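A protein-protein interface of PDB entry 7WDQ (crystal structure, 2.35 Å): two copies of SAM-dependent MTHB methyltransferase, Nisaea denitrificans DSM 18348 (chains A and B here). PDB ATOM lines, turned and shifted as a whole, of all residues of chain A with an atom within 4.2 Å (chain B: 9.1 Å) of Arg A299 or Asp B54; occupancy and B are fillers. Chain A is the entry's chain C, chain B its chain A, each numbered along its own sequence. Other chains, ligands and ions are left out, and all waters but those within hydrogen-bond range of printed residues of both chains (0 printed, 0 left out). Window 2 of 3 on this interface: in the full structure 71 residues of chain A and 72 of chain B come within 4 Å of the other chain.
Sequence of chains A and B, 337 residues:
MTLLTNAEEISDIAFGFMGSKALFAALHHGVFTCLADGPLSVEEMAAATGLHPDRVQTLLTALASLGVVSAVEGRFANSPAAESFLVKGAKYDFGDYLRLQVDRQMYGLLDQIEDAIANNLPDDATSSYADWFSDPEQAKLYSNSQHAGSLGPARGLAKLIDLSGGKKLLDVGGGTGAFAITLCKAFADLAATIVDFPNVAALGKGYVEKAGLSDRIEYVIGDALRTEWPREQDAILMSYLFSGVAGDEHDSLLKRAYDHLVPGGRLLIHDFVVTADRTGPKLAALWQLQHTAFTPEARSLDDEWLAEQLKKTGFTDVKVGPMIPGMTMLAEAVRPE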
ATOM      1  N   GLY A 247      -7.200  -5.755 -11.877  1.00  0.00           N
ATOM      2  CA  GLY A 247      -7.707  -4.405 -12.072  1.00  0.00           C
ATOM      3  C   GLY A 247      -8.334  -3.751 -10.855  1.00  0.00           C
ATOM      4  O   GLY A 247      -8.771  -2.598 -10.914  1.00  0.00           O
ATOM      5  N   GLU A 297      -7.405 -11.547 -14.124  1.00  0.00           N
ATOM      6  CA  GLU A 297      -8.176 -10.488 -13.476  1.00  0.00           C
ATOM      7  C   GLU A 297      -7.822  -9.102 -14.003  1.00  0.00           C
ATOM      8  O   GLU A 297      -8.346  -8.101 -13.523  1.00  0.00           O
ATOM      9  CB  GLU A 297      -7.999 -10.543 -11.954  1.00  0.00           C
ATOM     10  CG  GLU A 297      -8.578 -11.802 -11.317  1.00  0.00           C
ATOM     11  CD  GLU A 297      -9.375 -11.514 -10.053  1.00  0.00           C
ATOM     12  OE1 GLU A 297      -9.407 -10.344  -9.609  1.00  0.00           O
ATOM     13  OE2 GLU A 297      -9.981 -12.461  -9.509  1.00  0.00           O
ATOM     14  N   ALA A 298      -6.939  -9.058 -15.000  1.00  0.00           N
ATOM     15  CA  ALA A 298      -6.481  -7.805 -15.605  1.00  0.00           C
ATOM     16  C   ALA A 298      -7.610  -6.949 -16.174  1.00  0.00           C
ATOM     17  O   ALA A 298      -8.660  -7.458 -16.577  1.00  0.00           O
ATOM     18  CB  ALA A 298      -5.442  -8.090 -16.690  1.00  0.00           C
ATOM     19  N   ARG A 299      -7.382  -5.642 -16.190  1.00  0.00           N
ATOM     20  CA  ARG A 299      -8.323  -4.698 -16.769  1.00  0.00           C
ATOM     21  C   ARG A 299      -7.668  -3.973 -17.953  1.00  0.00           C
ATOM     22  O   ARG A 299      -6.465  -3.698 -17.934  1.00  0.00           O
ATOM     23  CB  ARG A 299      -8.747  -3.683 -15.714  1.00  0.00           C
ATOM     24  CG  ARG A 299     -10.211  -3.289 -15.791  1.00  0.00           C
ATOM     25  CD  ARG A 299     -10.449  -1.988 -15.057  1.00  0.00           C
ATOM     26  NE  ARG A 299      -9.824  -0.872 -15.762  1.00  0.00           N
ATOM     27  CZ  ARG A 299      -9.895   0.399 -15.376  1.00  0.00           C
ATOM     28  NH1 ARG A 299     -10.570   0.727 -14.278  1.00  0.00           N
ATOM     29  NH2 ARG A 299      -9.291   1.342 -16.090  1.00  0.00           N
ATOM     30  N   SER A 300      -8.458  -3.672 -18.983  1.00  0.00           N
ATOM     31  CA  SER A 300      -7.982  -2.876 -20.116  1.00  0.00           C
ATOM     32  C   SER A 300      -7.860  -1.404 -19.749  1.00  0.00           C
ATOM     33  O   SER A 300      -8.862  -0.745 -19.430  1.00  0.00           O
ATOM     34  CB  SER A 300      -8.910  -3.028 -21.325  1.00  0.00           C
ATOM     35  OG  SER A 300      -8.536  -2.144 -22.370  1.00  0.00           O
ATOM     36  N   LEU A 301      -6.627  -0.903 -19.805  1.00  0.00           N
ATOM     37  CA  LEU A 301      -6.314   0.501 -19.535  1.00  0.00           C
ATOM     38  C   LEU A 301      -6.516   1.422 -20.743  1.00  0.00           C
ATOM     39  O   LEU A 301      -5.876   1.241 -21.779  1.00  0.00           O
ATOM     40  CB  LEU A 301      -4.863   0.624 -19.088  1.00  0.00           C
ATOM     41  CG  LEU A 301      -4.593   0.668 -17.592  1.00  0.00           C
ATOM     42  CD1 LEU A 301      -4.992  -0.649 -16.949  1.00  0.00           C
ATOM     43  CD2 LEU A 301      -3.126   0.963 -17.377  1.00  0.00           C
ATOM     44  N   TRP A 305      -9.619   6.932 -18.795  1.00  0.00           N
ATOM     45  CA  TRP A 305      -9.828   6.429 -17.449  1.00  0.00           C
ATOM     46  C   TRP A 305      -8.636   6.845 -16.625  1.00  0.00           C
ATOM     47  O   TRP A 305      -8.769   7.335 -15.505  1.00  0.00           O
ATOM     48  CB  TRP A 305      -9.944   4.905 -17.412  1.00  0.00           C
ATOM     49  CG  TRP A 305      -9.957   4.422 -16.006  1.00  0.00           C
ATOM     50  CD1 TRP A 305     -11.044   4.283 -15.201  1.00  0.00           C
ATOM     51  CD2 TRP A 305      -8.818   4.069 -15.208  1.00  0.00           C
ATOM     52  NE1 TRP A 305     -10.659   3.849 -13.958  1.00  0.00           N
ATOM     53  CE2 TRP A 305      -9.296   3.708 -13.938  1.00  0.00           C
ATOM     54  CE3 TRP A 305      -7.443   4.015 -15.450  1.00  0.00           C
ATOM     55  CZ2 TRP A 305      -8.450   3.295 -12.908  1.00  0.00           C
ATOM     56  CZ3 TRP A 305      -6.600   3.603 -14.427  1.00  0.00           C
ATOM     57  CH2 TRP A 305      -7.108   3.252 -13.172  1.00  0.00           C
ATOM     58  N   VAL B  42     -20.483  -3.319 -23.949  1.00  0.00           N
ATOM     59  CA  VAL B  42     -19.673  -4.265 -23.204  1.00  0.00           C
ATOM     60  C   VAL B  42     -20.526  -5.077 -22.226  1.00  0.00           C
ATOM     61  O   VAL B  42     -20.475  -6.303 -22.237  1.00  0.00           O
ATOM     62  CB  VAL B  42     -18.490  -3.561 -22.494  1.00  0.00           C
ATOM     63  CG1 VAL B  42     -17.951  -4.413 -21.369  1.00  0.00           C
ATOM     64  CG2 VAL B  42     -17.381  -3.220 -23.513  1.00  0.00           C
ATOM     65  N   GLU B  43     -21.331  -4.404 -21.406  1.00  0.00           N
ATOM     66  CA  GLU B  43     -22.155  -5.107 -20.410  1.00  0.00           C
ATOM     67  C   GLU B  43     -23.267  -5.938 -21.046  1.00  0.00           C
ATOM     68  O   GLU B  43     -23.584  -7.028 -20.575  1.00  0.00           O
ATOM     69  CB  GLU B  43     -22.727  -4.151 -19.348  1.00  0.00           C
ATOM     70  CG  GLU B  43     -22.853  -2.696 -19.787  1.00  0.00           C
ATOM     71  CD  GLU B  43     -21.502  -1.963 -19.898  1.00  0.00           C
ATOM     72  OE1 GLU B  43     -20.673  -2.066 -18.955  1.00  0.00           O
ATOM     73  OE2 GLU B  43     -21.277  -1.281 -20.935  1.00  0.00           O
ATOM     74  N   MET B  45     -22.839  -7.365 -23.797  1.00  0.00           N
ATOM     75  CA  MET B  45     -22.031  -8.501 -24.223  1.00  0.00           C
ATOM     76  C   MET B  45     -21.652  -9.445 -23.064  1.00  0.00           C
ATOM     77  O   MET B  45     -21.716 -10.662 -23.209  1.00  0.00           O
ATOM     78  CB  MET B  45     -20.780  -8.010 -24.960  1.00  0.00           C
ATOM     79  CG  MET B  45     -20.898  -8.092 -26.468  1.00  0.00           C
ATOM     80  SD  MET B  45     -20.966  -9.820 -27.011  1.00  0.00           S
ATOM     81  CE  MET B  45     -19.309 -10.328 -26.547  1.00  0.00           C
ATOM     82  N   ALA B  46     -21.249  -8.875 -21.935  1.00  0.00           N
ATOM     83  CA  ALA B  46     -20.921  -9.649 -20.743  1.00  0.00           C
ATOM     84  C   ALA B  46     -22.108 -10.520 -20.327  1.00  0.00           C
ATOM     85  O   ALA B  46     -21.942 -11.637 -19.851  1.00  0.00           O
ATOM     86  CB  ALA B  46     -20.518  -8.723 -19.606  1.00  0.00           C
ATOM     87  N   LEU B  51     -19.209 -13.777 -19.876  1.00  0.00           N
ATOM     88  CA  LEU B  51     -17.867 -13.296 -19.579  1.00  0.00           C
ATOM     89  C   LEU B  51     -17.926 -12.057 -18.681  1.00  0.00           C
ATOM     90  O   LEU B  51     -18.904 -11.302 -18.703  1.00  0.00           O
ATOM     91  CB  LEU B  51     -17.103 -12.999 -20.870  1.00  0.00           C
ATOM     92  CG  LEU B  51     -16.804 -14.213 -21.752  1.00  0.00           C
ATOM     93  CD1 LEU B  51     -16.109 -13.785 -23.029  1.00  0.00           C
ATOM     94  CD2 LEU B  51     -15.958 -15.209 -20.997  1.00  0.00           C
ATOM     95  N   HIS B  52     -16.885 -11.857 -17.882  1.00  0.00           N
ATOM     96  CA  HIS B  52     -16.762 -10.646 -17.083  1.00  0.00           C
ATOM     97  C   HIS B  52     -16.577  -9.382 -17.953  1.00  0.00           C
ATOM     98  O   HIS B  52     -15.757  -9.377 -18.866  1.00  0.00           O
ATOM     99  CB  HIS B  52     -15.583 -10.779 -16.124  1.00  0.00           C
ATOM    100  CG  HIS B  52     -15.542  -9.704 -15.092  1.00  0.00           C
ATOM    101  ND1 HIS B  52     -15.243  -8.392 -15.398  1.00  0.00           N
ATOM    102  CD2 HIS B  52     -15.799  -9.734 -13.765  1.00  0.00           C
ATOM    103  CE1 HIS B  52     -15.299  -7.663 -14.298  1.00  0.00           C
ATOM    104  NE2 HIS B  52     -15.631  -8.454 -13.291  1.00  0.00           N
ATOM    105  N   PRO B  53     -17.315  -8.296 -17.643  1.00  0.00           N
ATOM    106  CA  PRO B  53     -17.272  -7.048 -18.417  1.00  0.00           C
ATOM    107  C   PRO B  53     -15.846  -6.605 -18.786  1.00  0.00           C
ATOM    108  O   PRO B  53     -15.610  -6.161 -19.907  1.00  0.00           O
ATOM    109  CB  PRO B  53     -17.912  -6.031 -17.464  1.00  0.00           C
ATOM    110  CG  PRO B  53     -18.823  -6.832 -16.624  1.00  0.00           C
ATOM    111  CD  PRO B  53     -18.141  -8.154 -16.428  1.00  0.00           C
ATOM    112  N   ASP B  54     -14.908  -6.742 -17.859  1.00  0.00           N
ATOM    113  CA  ASP B  54     -13.532  -6.351 -18.122  1.00  0.00           C
ATOM    114  C   ASP B  54     -12.778  -7.245 -19.133  1.00  0.00           C
ATOM    115  O   ASP B  54     -12.069  -6.733 -19.995  1.00  0.00           O
ATOM    116  CB  ASP B  54     -12.763  -6.205 -16.819  1.00  0.00           C
ATOM    117  CG  ASP B  54     -13.182  -4.972 -16.044  1.00  0.00           C
ATOM    118  OD1 ASP B  54     -13.664  -4.008 -16.690  1.00  0.00           O
ATOM    119  OD2 ASP B  54     -13.034  -4.965 -14.801  1.00  0.00           O
ATOM    120  N   ARG B  55     -12.925  -8.564 -19.047  1.00  0.00           N
ATOM    121  CA  ARG B  55     -12.324  -9.412 -20.065  1.00  0.00           C
ATOM    122  C   ARG B  55     -12.944  -9.168 -21.439  1.00  0.00           C
ATOM    123  O   ARG B  55     -12.217  -9.120 -22.442  1.00  0.00           O
ATOM    124  CB  ARG B  55     -12.392 -10.900 -19.701  1.00  0.00           C
ATOM    125  CG  ARG B  55     -11.346 -11.314 -18.698  1.00  0.00           C
ATOM    126  CD  ARG B  55     -11.867 -11.114 -17.268  1.00  0.00           C
ATOM    127  NE  ARG B  55     -11.221 -10.005 -16.592  1.00  0.00           N
ATOM    128  CZ  ARG B  55     -11.453  -9.651 -15.332  1.00  0.00           C
ATOM    129  NH1 ARG B  55     -12.331 -10.313 -14.591  1.00  0.00           N
ATOM    130  NH2 ARG B  55     -10.802  -8.619 -14.817  1.00  0.00           N
ATOM    131  N   VAL B  56     -14.271  -9.006 -21.502  1.00  0.00           N
ATOM    132  CA  VAL B  56     -14.915  -8.749 -22.790  1.00  0.00           C
ATOM    133  C   VAL B  56     -14.407  -7.439 -23.410  1.00  0.00           C
ATOM    134  O   VAL B  56     -14.217  -7.351 -24.623  1.00  0.00           O
ATOM    135  CB  VAL B  56     -16.459  -8.718 -22.722  1.00  0.00           C
ATOM    136  CG1 VAL B  56     -16.995  -9.762 -21.759  1.00  0.00           C
ATOM    137  CG2 VAL B  56     -16.936  -7.344 -22.336  1.00  0.00           C
ATOM    138  N   GLN B  57     -14.180  -6.432 -22.576  1.00  0.00           N
ATOM    139  CA  GLN B  57     -13.659  -5.160 -23.053  1.00  0.00           C
ATOM    140  C   GLN B  57     -12.292  -5.356 -23.697  1.00  0.00           C
ATOM    141  O   GLN B  57     -12.069  -4.919 -24.826  1.00  0.00           O
ATOM    142  CB  GLN B  57     -13.554  -4.177 -21.903  1.00  0.00           C
ATOM    143  CG  GLN B  57     -13.016  -2.817 -22.256  1.00  0.00           C
ATOM    144  CD  GLN B  57     -13.243  -1.839 -21.118  1.00  0.00           C
ATOM    145  OE1 GLN B  57     -14.061  -0.922 -21.231  1.00  0.00           O
ATOM    146  NE2 GLN B  57     -12.544  -2.051 -19.995  1.00  0.00           N
ATOM    147  N   THR B  58     -11.399  -6.037 -22.980  1.00  0.00           N
ATOM    148  CA  THR B  58     -10.070  -6.354 -23.482  1.00  0.00           C
ATOM    149  C   THR B  58     -10.115  -7.128 -24.794  1.00  0.00           C
ATOM    150  O   THR B  58      -9.417  -6.782 -25.733  1.00  0.00           O
ATOM    151  CB  THR B  58      -9.240  -7.131 -22.441  1.00  0.00           C
ATOM    152  OG1 THR B  58      -8.975  -6.279 -21.326  1.00  0.00           O
ATOM    153  CG2 THR B  58      -7.912  -7.571 -23.028  1.00  0.00           C
ATOM    154  N   LEU B  59     -10.951  -8.158 -24.859  1.00  0.00           N
ATOM    155  CA  LEU B  59     -11.081  -8.966 -26.066  1.00  0.00           C
ATOM    156  C   LEU B  59     -11.668  -8.198 -27.262  1.00  0.00           C
ATOM    157  O   LEU B  59     -11.177  -8.317 -28.371  1.00  0.00           O
ATOM    158  CB  LEU B  59     -11.918 -10.209 -25.789  1.00  0.00           C
ATOM    159  CG  LEU B  59     -12.033 -11.215 -26.935  1.00  0.00           C
ATOM    160  CD1 LEU B  59     -10.654 -11.694 -27.434  1.00  0.00           C
ATOM    161  CD2 LEU B  59     -12.874 -12.389 -26.495  1.00  0.00           C
ATOM    162  N   LEU B  60     -12.719  -7.421 -27.031  1.00  0.00           N
ATOM    163  CA  LEU B  60     -13.354  -6.638 -28.090  1.00  0.00           C
ATOM    164  C   LEU B  60     -12.464  -5.479 -28.579  1.00  0.00           C
ATOM    165  O   LEU B  60     -12.386  -5.193 -29.778  1.00  0.00           O
ATOM    166  CB  LEU B  60     -14.722  -6.113 -27.630  1.00  0.00           C
ATOM    167  CG  LEU B  60     -15.934  -7.052 -27.728  1.00  0.00           C
ATOM    168  CD1 LEU B  60     -16.420  -7.180 -29.174  1.00  0.00           C
ATOM    169  CD2 LEU B  60     -15.618  -8.424 -27.165  1.00  0.00           C
ATOM    170  N   THR B  61     -11.783  -4.814 -27.660  1.00  0.00           N
ATOM    171  CA  THR B  61     -10.843  -3.775 -28.066  1.00  0.00           C
ATOM    172  C   THR B  61      -9.806  -4.354 -29.027  1.00  0.00           C
ATOM    173  O   THR B  61      -9.514  -3.759 -30.069  1.00  0.00           O
ATOM    174  CB  THR B  61     -10.160  -3.132 -26.859  1.00  0.00           C
ATOM    175  OG1 THR B  61     -11.161  -2.519 -26.045  1.00  0.00           O
ATOM    176  CG2 THR B  61      -9.165  -2.060 -27.291  1.00  0.00           C
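The backbone carbonyl oxygen of Ala A298 lies within hydrogen-bond range of the guanidinium group of Arg B55, 3.0 Å away.
The backbone carbonyl oxygen (O) of Glu A297 sits at hydrogen-bond distance from the guanidinium group (NH2) of Arg B55 (2.8 Å).
The side-chain hydroxyl (OG1) of Thr B61 is in hydrogen-bond range of the backbone carbonyl oxygen (O) of Gln B57, 2.8 Å away.
The backbone NH (N) of Gly A247 lies within hydrogen-bond range of the backbone carbonyl oxygen (O) of Glu A297, 3.1 Å away.
ND1 of His B52 lies within hydrogen-bond range of N of Asp B54.
The backbone carbonyl oxygen (O) of Asp B54 lies within hydrogen-bond range of the side-chain hydroxyl (OG1) of Thr B58 (3.4 Å).
Among the printed residues, pairs that only touch across the chains: Ser A300 with Thr B58, Arg A299 with Asp B54 and Ser A300 with Gln B57.
Arg A299 touches just one residue of chain B: Asp B54 (3.4 Å).
Asp B54 touches one residue of chain A.
No residue of chain B comes within 4 Å of Gly A247.
Of the printed residues of chain B, Glu A297 touches Arg B55.
Of the printed residues of chain A, Gln B57 touches Ser A300 (3.9 Å).
Of the printed residues of chain A, Thr B58 touches Ser A300 (3.3 Å).
Of the printed residues of chain A, Arg B55 touches Glu A297 (2.8 Å) and Ala A298 (3.0 Å).
Leu B60 touches none of the printed residues of chain A.
The nearest residue of chain B that does not touch Arg A299 is Thr B58 (4.3 Å).
The nearest printed residue of chain A that does not touch Gln B57 is Arg A299 (5.0 Å).
Printed residues of chain B that touch a printed residue of chain A: Asp B54, Arg B55, Gln B57 and Thr B58.
Among the printed residues, 5 pairs touch across the chains.
Among the printed residues, no Asp or Glu carboxylate lies within 4 Å of a Lys or Arg side-chain nitrogen of the other chain.
No position is printed for both chains.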
